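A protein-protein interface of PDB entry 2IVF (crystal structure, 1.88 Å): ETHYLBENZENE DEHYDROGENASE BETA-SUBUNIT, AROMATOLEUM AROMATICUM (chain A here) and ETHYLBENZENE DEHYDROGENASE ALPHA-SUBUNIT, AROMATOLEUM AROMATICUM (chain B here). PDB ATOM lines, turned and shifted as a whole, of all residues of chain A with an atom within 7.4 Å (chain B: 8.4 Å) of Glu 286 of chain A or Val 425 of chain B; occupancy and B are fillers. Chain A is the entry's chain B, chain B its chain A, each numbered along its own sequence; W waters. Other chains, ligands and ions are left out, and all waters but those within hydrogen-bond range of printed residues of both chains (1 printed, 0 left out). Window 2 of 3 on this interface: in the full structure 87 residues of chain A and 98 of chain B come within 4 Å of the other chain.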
ATOM      1  N   ASN A 141      30.526  29.349  -9.100  1.00  0.00           N
ATOM      2  CA  ASN A 141      31.723  29.505  -9.895  1.00  0.00           C
ATOM      3  C   ASN A 141      33.000  29.075  -9.198  1.00  0.00           C
ATOM      4  O   ASN A 141      34.001  29.791  -9.236  1.00  0.00           O
ATOM      5  CB  ASN A 141      31.895  30.962 -10.350  1.00  0.00           C
ATOM      6  CG  ASN A 141      30.849  31.382 -11.339  1.00  0.00           C
ATOM      7  OD1 ASN A 141      30.686  30.721 -12.346  1.00  0.00           O
ATOM      8  ND2 ASN A 141      30.076  32.447 -11.015  1.00  0.00           N
ATOM      9  N   GLY A 280      31.612  30.204 -16.807  1.00  0.00           N
ATOM     10  CA  GLY A 280      31.007  30.546 -15.531  1.00  0.00           C
ATOM     11  C   GLY A 280      29.599  31.082 -15.678  1.00  0.00           C
ATOM     12  O   GLY A 280      29.094  31.389 -16.780  1.00  0.00           O
ATOM     13  N   PHE A 281      28.987  31.259 -14.523  1.00  0.00           N
ATOM     14  CA  PHE A 281      27.679  31.857 -14.430  1.00  0.00           C
ATOM     15  C   PHE A 281      27.822  33.301 -14.032  1.00  0.00           C
ATOM     16  O   PHE A 281      28.713  33.624 -13.254  1.00  0.00           O
ATOM     17  CB  PHE A 281      26.896  31.096 -13.375  1.00  0.00           C
ATOM     18  CG  PHE A 281      26.713  29.696 -13.740  1.00  0.00           C
ATOM     19  CD1 PHE A 281      25.670  29.326 -14.567  1.00  0.00           C
ATOM     20  CD2 PHE A 281      27.593  28.743 -13.285  1.00  0.00           C
ATOM     21  CE1 PHE A 281      25.543  27.990 -14.937  1.00  0.00           C
ATOM     22  CE2 PHE A 281      27.466  27.418 -13.640  1.00  0.00           C
ATOM     23  CZ  PHE A 281      26.434  27.041 -14.441  1.00  0.00           C
ATOM     24  N   GLY A 282      26.946  34.158 -14.556  1.00  0.00           N
ATOM     25  CA  GLY A 282      26.977  35.572 -14.250  1.00  0.00           C
ATOM     26  C   GLY A 282      26.323  35.903 -12.934  1.00  0.00           C
ATOM     27  O   GLY A 282      25.733  35.019 -12.250  1.00  0.00           O
ATOM     28  N   GLU A 283      26.313  37.197 -12.638  1.00  0.00           N
ATOM     29  CA  GLU A 283      25.673  37.723 -11.409  1.00  0.00           C
ATOM     30  C   GLU A 283      24.186  37.432 -11.408  1.00  0.00           C
ATOM     31  O   GLU A 283      23.552  37.327 -10.320  1.00  0.00           O
ATOM     32  CB  GLU A 283      25.891  39.232 -11.295  1.00  0.00           C
ATOM     33  CG  GLU A 283      27.342  39.574 -11.058  1.00  0.00           C
ATOM     34  CD  GLU A 283      27.548  41.061 -10.991  1.00  0.00           C
ATOM     35  OE1 GLU A 283      26.731  41.815 -11.595  1.00  0.00           O
ATOM     36  OE2 GLU A 283      28.526  41.448 -10.311  1.00  0.00           O
ATOM     37  N   ASP A 284      23.628  37.287 -12.615  1.00  0.00           N
ATOM     38  CA  ASP A 284      22.224  36.938 -12.751  1.00  0.00           C
ATOM     39  C   ASP A 284      21.902  35.477 -12.662  1.00  0.00           C
ATOM     40  O   ASP A 284      20.753  35.095 -12.752  1.00  0.00           O
ATOM     41  CB  ASP A 284      21.648  37.510 -14.042  1.00  0.00           C
ATOM     42  CG  ASP A 284      22.278  36.935 -15.285  1.00  0.00           C
ATOM     43  OD1 ASP A 284      23.178  36.073 -15.208  1.00  0.00           O
ATOM     44  OD2 ASP A 284      21.848  37.379 -16.357  1.00  0.00           O
ATOM     45  N   GLY A 285      22.925  34.685 -12.496  1.00  0.00           N
ATOM     46  CA  GLY A 285      22.832  33.245 -12.367  1.00  0.00           C
ATOM     47  C   GLY A 285      22.764  32.511 -13.702  1.00  0.00           C
ATOM     48  O   GLY A 285      22.738  31.279 -13.727  1.00  0.00           O
ATOM     49  N   GLU A 286      22.794  33.252 -14.819  1.00  0.00           N
ATOM     50  CA  GLU A 286      22.710  32.639 -16.130  1.00  0.00           C
ATOM     51  C   GLU A 286      24.096  32.292 -16.663  1.00  0.00           C
ATOM     52  O   GLU A 286      25.158  32.816 -16.227  1.00  0.00           O
ATOM     53  CB  GLU A 286      21.941  33.543 -17.126  1.00  0.00           C
ATOM     54  CG  GLU A 286      20.486  33.928 -16.734  1.00  0.00           C
ATOM     55  CD  GLU A 286      19.522  32.767 -16.688  1.00  0.00           C
ATOM     56  OE1 GLU A 286      19.814  31.694 -17.258  1.00  0.00           O
ATOM     57  OE2 GLU A 286      18.462  32.899 -16.016  1.00  0.00           O
ATOM     58  N   ILE A 287      24.127  31.380 -17.620  1.00  0.00           N
ATOM     59  CA  ILE A 287      25.396  30.963 -18.178  1.00  0.00           C
ATOM     60  C   ILE A 287      26.019  32.119 -19.018  1.00  0.00           C
ATOM     61  O   ILE A 287      25.321  32.864 -19.685  1.00  0.00           O
ATOM     62  CB  ILE A 287      25.258  29.648 -18.999  1.00  0.00           C
ATOM     63  CG1 ILE A 287      26.622  29.053 -19.285  1.00  0.00           C
ATOM     64  CG2 ILE A 287      24.491  29.903 -20.314  1.00  0.00           C
ATOM     65  CD1 ILE A 287      27.427  28.565 -18.035  1.00  0.00           C
ATOM     66  N   THR A 288      27.338  32.274 -18.944  1.00  0.00           N
ATOM     67  CA  THR A 288      28.010  33.331 -19.680  1.00  0.00           C
ATOM     68  C   THR A 288      28.848  32.669 -20.791  1.00  0.00           C
ATOM     69  O   THR A 288      28.905  31.435 -20.896  1.00  0.00           O
ATOM     70  CB  THR A 288      28.959  34.187 -18.789  1.00  0.00           C
ATOM     71  OG1 THR A 288      30.154  33.438 -18.516  1.00  0.00           O
ATOM     72  CG2 THR A 288      28.295  34.622 -17.467  1.00  0.00           C
ATOM     73  N   ASP A 289      29.525  33.494 -21.575  1.00  0.00           N
ATOM     74  CA  ASP A 289      30.418  32.985 -22.628  1.00  0.00           C
ATOM     75  C   ASP A 289      31.867  33.003 -22.192  1.00  0.00           C
ATOM     76  O   ASP A 289      32.761  32.844 -23.029  1.00  0.00           O
ATOM     77  CB  ASP A 289      30.262  33.838 -23.907  1.00  0.00           C
ATOM     78  CG  ASP A 289      30.570  35.323 -23.693  1.00  0.00           C
ATOM     79  OD1 ASP A 289      30.870  35.757 -22.568  1.00  0.00           O
ATOM     80  OD2 ASP A 289      30.522  36.081 -24.673  1.00  0.00           O
ATOM     81  N   PHE B 306      16.123  18.223 -15.861  1.00  0.00           N
ATOM     82  CA  PHE B 306      17.031  18.864 -16.828  1.00  0.00           C
ATOM     83  C   PHE B 306      16.747  18.308 -18.213  1.00  0.00           C
ATOM     84  O   PHE B 306      16.507  19.048 -19.166  1.00  0.00           O
ATOM     85  CB  PHE B 306      18.491  18.721 -16.413  1.00  0.00           C
ATOM     86  CG  PHE B 306      19.474  19.090 -17.512  1.00  0.00           C
ATOM     87  CD1 PHE B 306      19.774  20.420 -17.799  1.00  0.00           C
ATOM     88  CD2 PHE B 306      20.066  18.111 -18.269  1.00  0.00           C
ATOM     89  CE1 PHE B 306      20.646  20.737 -18.838  1.00  0.00           C
ATOM     90  CE2 PHE B 306      20.906  18.429 -19.297  1.00  0.00           C
ATOM     91  CZ  PHE B 306      21.203  19.746 -19.575  1.00  0.00           C
ATOM     92  N   GLY B 309      13.448  19.217 -19.646  1.00  0.00           N
ATOM     93  CA  GLY B 309      13.535  20.615 -20.095  1.00  0.00           C
ATOM     94  C   GLY B 309      14.137  20.701 -21.486  1.00  0.00           C
ATOM     95  O   GLY B 309      13.613  21.418 -22.369  1.00  0.00           O
ATOM     96  N   LEU B 310      15.198  19.933 -21.714  1.00  0.00           N
ATOM     97  CA  LEU B 310      15.831  19.863 -23.028  1.00  0.00           C
ATOM     98  C   LEU B 310      14.849  19.321 -24.069  1.00  0.00           C
ATOM     99  O   LEU B 310      14.801  19.794 -25.195  1.00  0.00           O
ATOM    100  CB  LEU B 310      17.088  18.997 -23.006  1.00  0.00           C
ATOM    101  CG  LEU B 310      18.436  19.730 -22.831  1.00  0.00           C
ATOM    102  CD1 LEU B 310      18.468  20.718 -21.658  1.00  0.00           C
ATOM    103  CD2 LEU B 310      19.602  18.742 -22.806  1.00  0.00           C
ATOM    104  N   VAL B 313      12.285  21.866 -24.950  1.00  0.00           N
ATOM    105  CA  VAL B 313      12.871  22.849 -25.862  1.00  0.00           C
ATOM    106  C   VAL B 313      12.817  22.379 -27.313  1.00  0.00           C
ATOM    107  O   VAL B 313      12.331  23.102 -28.191  1.00  0.00           O
ATOM    108  CB  VAL B 313      14.278  23.220 -25.440  1.00  0.00           C
ATOM    109  CG1 VAL B 313      15.020  24.023 -26.561  1.00  0.00           C
ATOM    110  CG2 VAL B 313      14.240  23.998 -24.158  1.00  0.00           C
ATOM    111  N   THR B 413       8.807  23.223 -18.959  1.00  0.00           N
ATOM    112  CA  THR B 413       9.329  24.345 -19.711  1.00  0.00           C
ATOM    113  C   THR B 413      10.665  24.688 -19.033  1.00  0.00           C
ATOM    114  O   THR B 413      10.914  24.310 -17.891  1.00  0.00           O
ATOM    115  CB  THR B 413       8.368  25.543 -19.657  1.00  0.00           C
ATOM    116  OG1 THR B 413       8.254  25.985 -18.287  1.00  0.00           O
ATOM    117  CG2 THR B 413       6.968  25.138 -20.219  1.00  0.00           C
ATOM    118  N   PRO B 414      11.556  25.354 -19.739  1.00  0.00           N
ATOM    119  CA  PRO B 414      12.834  25.650 -19.095  1.00  0.00           C
ATOM    120  C   PRO B 414      12.745  26.380 -17.759  1.00  0.00           C
ATOM    121  O   PRO B 414      13.503  26.094 -16.852  1.00  0.00           O
ATOM    122  CB  PRO B 414      13.547  26.505 -20.140  1.00  0.00           C
ATOM    123  CG  PRO B 414      12.975  26.076 -21.421  1.00  0.00           C
ATOM    124  CD  PRO B 414      11.525  25.816 -21.132  1.00  0.00           C
ATOM    125  N   GLU B 415      11.845  27.334 -17.652  1.00  0.00           N
ATOM    126  CA  GLU B 415      11.589  28.018 -16.406  1.00  0.00           C
ATOM    127  C   GLU B 415      11.193  27.015 -15.335  1.00  0.00           C
ATOM    128  O   GLU B 415      11.726  27.024 -14.239  1.00  0.00           O
ATOM    129  CB  GLU B 415      10.470  29.048 -16.596  1.00  0.00           C
ATOM    130  CG  GLU B 415      10.854  30.227 -17.499  1.00  0.00           C
ATOM    131  CD  GLU B 415      10.835  29.918 -19.009  1.00  0.00           C
ATOM    132  OE1 GLU B 415      10.306  28.861 -19.445  1.00  0.00           O
ATOM    133  OE2 GLU B 415      11.360  30.769 -19.760  1.00  0.00           O
ATOM    134  N   LYS B 416      10.254  26.128 -15.651  1.00  0.00           N
ATOM    135  CA  LYS B 416       9.803  25.145 -14.658  1.00  0.00           C
ATOM    136  C   LYS B 416      10.840  24.072 -14.353  1.00  0.00           C
ATOM    137  O   LYS B 416      11.054  23.723 -13.189  1.00  0.00           O
ATOM    138  CB  LYS B 416       8.510  24.519 -15.138  1.00  0.00           C
ATOM    139  CG  LYS B 416       7.421  25.514 -15.167  1.00  0.00           C
ATOM    140  CD  LYS B 416       6.119  24.882 -15.613  1.00  0.00           C
ATOM    141  CE  LYS B 416       5.056  25.924 -15.895  1.00  0.00           C
ATOM    142  NZ  LYS B 416       3.777  25.261 -16.332  1.00  0.00           N
ATOM    143  N   ALA B 417      11.534  23.587 -15.386  1.00  0.00           N
ATOM    144  CA  ALA B 417      12.551  22.564 -15.221  1.00  0.00           C
ATOM    145  C   ALA B 417      13.681  23.162 -14.375  1.00  0.00           C
ATOM    146  O   ALA B 417      14.197  22.513 -13.475  1.00  0.00           O
ATOM    147  CB  ALA B 417      13.080  22.132 -16.558  1.00  0.00           C
ATOM    148  N   SER B 418      14.042  24.416 -14.658  1.00  0.00           N
ATOM    149  CA  SER B 418      15.056  25.126 -13.869  1.00  0.00           C
ATOM    150  C   SER B 418      14.695  25.186 -12.377  1.00  0.00           C
ATOM    151  O   SER B 418      15.552  25.001 -11.523  1.00  0.00           O
ATOM    152  CB  SER B 418      15.238  26.539 -14.401  1.00  0.00           C
ATOM    153  OG  SER B 418      16.075  27.284 -13.545  1.00  0.00           O
ATOM    154  N   ALA B 419      13.443  25.448 -12.066  1.00  0.00           N
ATOM    155  CA  ALA B 419      12.994  25.471 -10.665  1.00  0.00           C
ATOM    156  C   ALA B 419      13.218  24.115 -10.045  1.00  0.00           C
ATOM    157  O   ALA B 419      13.544  24.028  -8.869  1.00  0.00           O
ATOM    158  CB  ALA B 419      11.539  25.874 -10.558  1.00  0.00           C
ATOM    159  N   CYS B 421      15.502  21.585 -11.116  1.00  0.00           N
ATOM    160  CA  CYS B 421      16.846  21.038 -11.058  1.00  0.00           C
ATOM    161  C   CYS B 421      17.961  22.038 -10.750  1.00  0.00           C
ATOM    162  O   CYS B 421      19.136  21.649 -10.630  1.00  0.00           O
ATOM    163  CB  CYS B 421      17.201  20.333 -12.362  1.00  0.00           C
ATOM    164  SG  CYS B 421      17.359  21.435 -13.826  1.00  0.00           S
ATOM    165  N   GLY B 422      17.599  23.305 -10.621  1.00  0.00           N
ATOM    166  CA  GLY B 422      18.563  24.337 -10.291  1.00  0.00           C
ATOM    167  C   GLY B 422      19.508  24.737 -11.406  1.00  0.00           C
ATOM    168  O   GLY B 422      20.417  25.526 -11.192  1.00  0.00           O
ATOM    169  N   VAL B 423      19.280  24.245 -12.617  1.00  0.00           N
ATOM    170  CA  VAL B 423      20.111  24.630 -13.769  1.00  0.00           C
ATOM    171  C   VAL B 423      19.476  25.882 -14.358  1.00  0.00           C
ATOM    172  O   VAL B 423      18.256  25.937 -14.490  1.00  0.00           O
ATOM    173  CB  VAL B 423      20.140  23.484 -14.794  1.00  0.00           C
ATOM    174  CG1 VAL B 423      21.017  23.832 -16.004  1.00  0.00           C
ATOM    175  CG2 VAL B 423      20.669  22.232 -14.119  1.00  0.00           C
ATOM    176  N   PRO B 424      20.278  26.922 -14.661  1.00  0.00           N
ATOM    177  CA  PRO B 424      19.711  28.151 -15.201  1.00  0.00           C
ATOM    178  C   PRO B 424      18.948  27.891 -16.502  1.00  0.00           C
ATOM    179  O   PRO B 424      19.340  27.030 -17.309  1.00  0.00           O
ATOM    180  CB  PRO B 424      20.956  29.041 -15.465  1.00  0.00           C
ATOM    181  CG  PRO B 424      21.987  28.496 -14.653  1.00  0.00           C
ATOM    182  CD  PRO B 424      21.743  27.016 -14.488  1.00  0.00           C
ATOM    183  N   VAL B 425      17.846  28.604 -16.690  1.00  0.00           N
ATOM    184  CA  VAL B 425      17.081  28.588 -17.948  1.00  0.00           C
ATOM    185  C   VAL B 425      17.937  28.733 -19.219  1.00  0.00           C
ATOM    186  O   VAL B 425      17.733  28.010 -20.226  1.00  0.00           O
ATOM    187  CB  VAL B 425      16.021  29.695 -17.927  1.00  0.00           C
ATOM    188  CG1 VAL B 425      15.343  29.838 -19.283  1.00  0.00           C
ATOM    189  CG2 VAL B 425      14.983  29.396 -16.811  1.00  0.00           C
ATOM    190  N   SER B 426      18.903  29.638 -19.166  1.00  0.00           N
ATOM    191  CA  SER B 426      19.756  29.930 -20.316  1.00  0.00           C
ATOM    192  C   SER B 426      20.474  28.672 -20.770  1.00  0.00           C
ATOM    193  O   SER B 426      20.625  28.409 -21.957  1.00  0.00           O
ATOM    194  CB  SER B 426      20.750  31.050 -19.975  1.00  0.00           C
ATOM    195  OG  SER B 426      21.550  30.755 -18.815  1.00  0.00           O
ATOM    196  N   LEU B 427      20.917  27.893 -19.804  1.00  0.00           N
ATOM    197  CA  LEU B 427      21.686  26.691 -20.076  1.00  0.00           C
ATOM    198  C   LEU B 427      20.800  25.524 -20.542  1.00  0.00           C
ATOM    199  O   LEU B 427      21.187  24.721 -21.383  1.00  0.00           O
ATOM    200  CB  LEU B 427      22.473  26.337 -18.801  1.00  0.00           C
ATOM    201  CG  LEU B 427      23.584  25.320 -18.866  1.00  0.00           C
ATOM    202  CD1 LEU B 427      24.493  25.526 -20.145  1.00  0.00           C
ATOM    203  CD2 LEU B 427      24.402  25.324 -17.569  1.00  0.00           C
ATOM    204  N   ILE B 428      19.624  25.404 -19.955  1.00  0.00           N
ATOM    205  CA  ILE B 428      18.623  24.458 -20.432  1.00  0.00           C
ATOM    206  C   ILE B 428      18.294  24.743 -21.917  1.00  0.00           C
ATOM    207  O   ILE B 428      18.331  23.834 -22.776  1.00  0.00           O
ATOM    208  CB  ILE B 428      17.362  24.535 -19.588  1.00  0.00           C
ATOM    209  CG1 ILE B 428      17.669  24.055 -18.149  1.00  0.00           C
ATOM    210  CG2 ILE B 428      16.216  23.731 -20.289  1.00  0.00           C
ATOM    211  CD1 ILE B 428      16.419  24.049 -17.137  1.00  0.00           C
ATOM    212  N   ARG B 429      18.028  26.007 -22.229  1.00  0.00           N
ATOM    213  CA  ARG B 429      17.664  26.368 -23.602  1.00  0.00           C
ATOM    214  C   ARG B 429      18.846  26.190 -24.548  1.00  0.00           C
ATOM    215  O   ARG B 429      18.683  25.626 -25.636  1.00  0.00           O
ATOM    216  CB  ARG B 429      17.099  27.781 -23.673  1.00  0.00           C
ATOM    217  CG  ARG B 429      16.174  27.988 -24.877  1.00  0.00           C
ATOM    218  CD  ARG B 429      15.268  29.166 -24.731  1.00  0.00           C
ATOM    219  NE  ARG B 429      14.022  28.914 -24.020  1.00  0.00           N
ATOM    220  CZ  ARG B 429      13.545  29.682 -23.036  1.00  0.00           C
ATOM    221  NH1 ARG B 429      14.217  30.746 -22.573  1.00  0.00           N
ATOM    222  NH2 ARG B 429      12.380  29.368 -22.489  1.00  0.00           N
ATOM    223  N   GLU B 430      20.040  26.636 -24.136  1.00  0.00           N
ATOM    224  CA  GLU B 430      21.233  26.441 -24.960  1.00  0.00           C
ATOM    225  C   GLU B 430      21.524  24.977 -25.287  1.00  0.00           C
ATOM    226  O   GLU B 430      21.794  24.631 -26.436  1.00  0.00           O
ATOM    227  CB  GLU B 430      22.472  27.010 -24.286  1.00  0.00           C
ATOM    228  CG  GLU B 430      23.731  26.897 -25.144  1.00  0.00           C
ATOM    229  CD  GLU B 430      24.943  27.517 -24.444  1.00  0.00           C
ATOM    230  OE1 GLU B 430      24.743  28.540 -23.754  1.00  0.00           O
ATOM    231  OE2 GLU B 430      26.034  26.950 -24.591  1.00  0.00           O
ATOM    232  N   LEU B 431      21.500  24.131 -24.266  1.00  0.00           N
ATOM    233  CA  LEU B 431      21.758  22.732 -24.457  1.00  0.00           C
ATOM    234  C   LEU B 431      20.629  21.984 -25.173  1.00  0.00           C
ATOM    235  O   LEU B 431      20.903  21.016 -25.905  1.00  0.00           O
ATOM    236  CB  LEU B 431      22.145  22.057 -23.141  1.00  0.00           C
ATOM    237  CG  LEU B 431      23.525  22.497 -22.614  1.00  0.00           C
ATOM    238  CD1 LEU B 431      23.831  22.013 -21.147  1.00  0.00           C
ATOM    239  CD2 LEU B 431      24.681  22.077 -23.587  1.00  0.00           C
ATOM    240  N   GLY B 432      19.383  22.409 -24.972  1.00  0.00           N
ATOM    241  CA  GLY B 432      18.257  21.897 -25.769  1.00  0.00           C
ATOM    242  C   GLY B 432      18.526  22.041 -27.244  1.00  0.00           C
ATOM    243  O   GLY B 432      18.372  21.095 -28.035  1.00  0.00           O
HETATM  244  O   HOH W   1      17.565  30.756 -14.730  1.00  0.00           O
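OG of Ser 426 of chain B is in hydrogen-bond range of OE1 of Glu 286 of chain A, at 2.5 Å. OG of Ser 426 of chain B lies within hydrogen-bond range of N of Ile 287 of chain A (2.9 Å).
OD1 of Asn 141 of chain A lies within hydrogen-bond range of N of Phe 281 of chain A, 2.8 Å away. The backbone NH of Glu 286 of chain A lies within hydrogen-bond range of the side-chain carboxylate of Asp 284 of chain A (2.9 Å).
CE1 of Phe 281 of chain A touches CG of Pro 424 of chain B, at 3.6 Å. CE1 of Phe 281 of chain A touches CD2 of Leu 427 of chain B, 3.9 Å away. Gly 285 of chain A touches Pro 424 of chain B. Pro 424 of chain B touches Glu 286 of chain A. OE1 of Glu 286 of chain A touches N of Val 425 of chain B, 3.7 Å away. Glu 430 of chain B touches Ile 287 of chain A.
Of chain B, only Pro 424 (3.0 Å) comes within 4 Å of Gly 285 of chain A. Glu 286 of chain A touches just these residues of chain B: Pro 424 (3.4 Å), Val 425 (3.7 Å) and Ser 426 (2.5 Å). Printed residues of chain B within 4 Å of Ile 287 of chain A: Ser 426 (2.9 Å) and Glu 430 (3.7 Å). Printed residues of chain A within 4 Å of Pro 424 of chain B: Phe 281, Gly 285 and Glu 286. Of chain A, only Glu 286 (3.7 Å) comes within 4 Å of Val 425 of chain B. Of the printed residues of chain A, Ser 426 of chain B touches Glu 286 and Ile 287. Printed residues of chain A within 4 Å of Leu 427 of chain B: Phe 281 (3.9 Å). Printed residues of chain A within 4 Å of Glu 430 of chain B: Ile 287 (3.7 Å).
Printed residues of chain A that touch a printed residue of chain B: Phe 281, Gly 285, Glu 286 and Ile 287. Hydrophobic or aromatic side chains of chain A within 4 Å of the printed part of chain B: Phe 281 and Ile 287. Along chain A the printed residues that touch a printed residue of chain B span positions 281 to 287. Printed residues of chain B that touch a printed residue of chain A: Pro 424, Val 425, Ser 426, Leu 427 and Glu 430. Among the printed residues, 8 pairs touch across the chains. Among the printed residues, no Asp or Glu carboxylate lies within 4 Å of a Lys or Arg side-chain nitrogen of the other chain.
Water W1 bridges OE2 of Glu 286 of chain A (2.7 Å) and N of Val 425 of chain B (2.9 Å).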
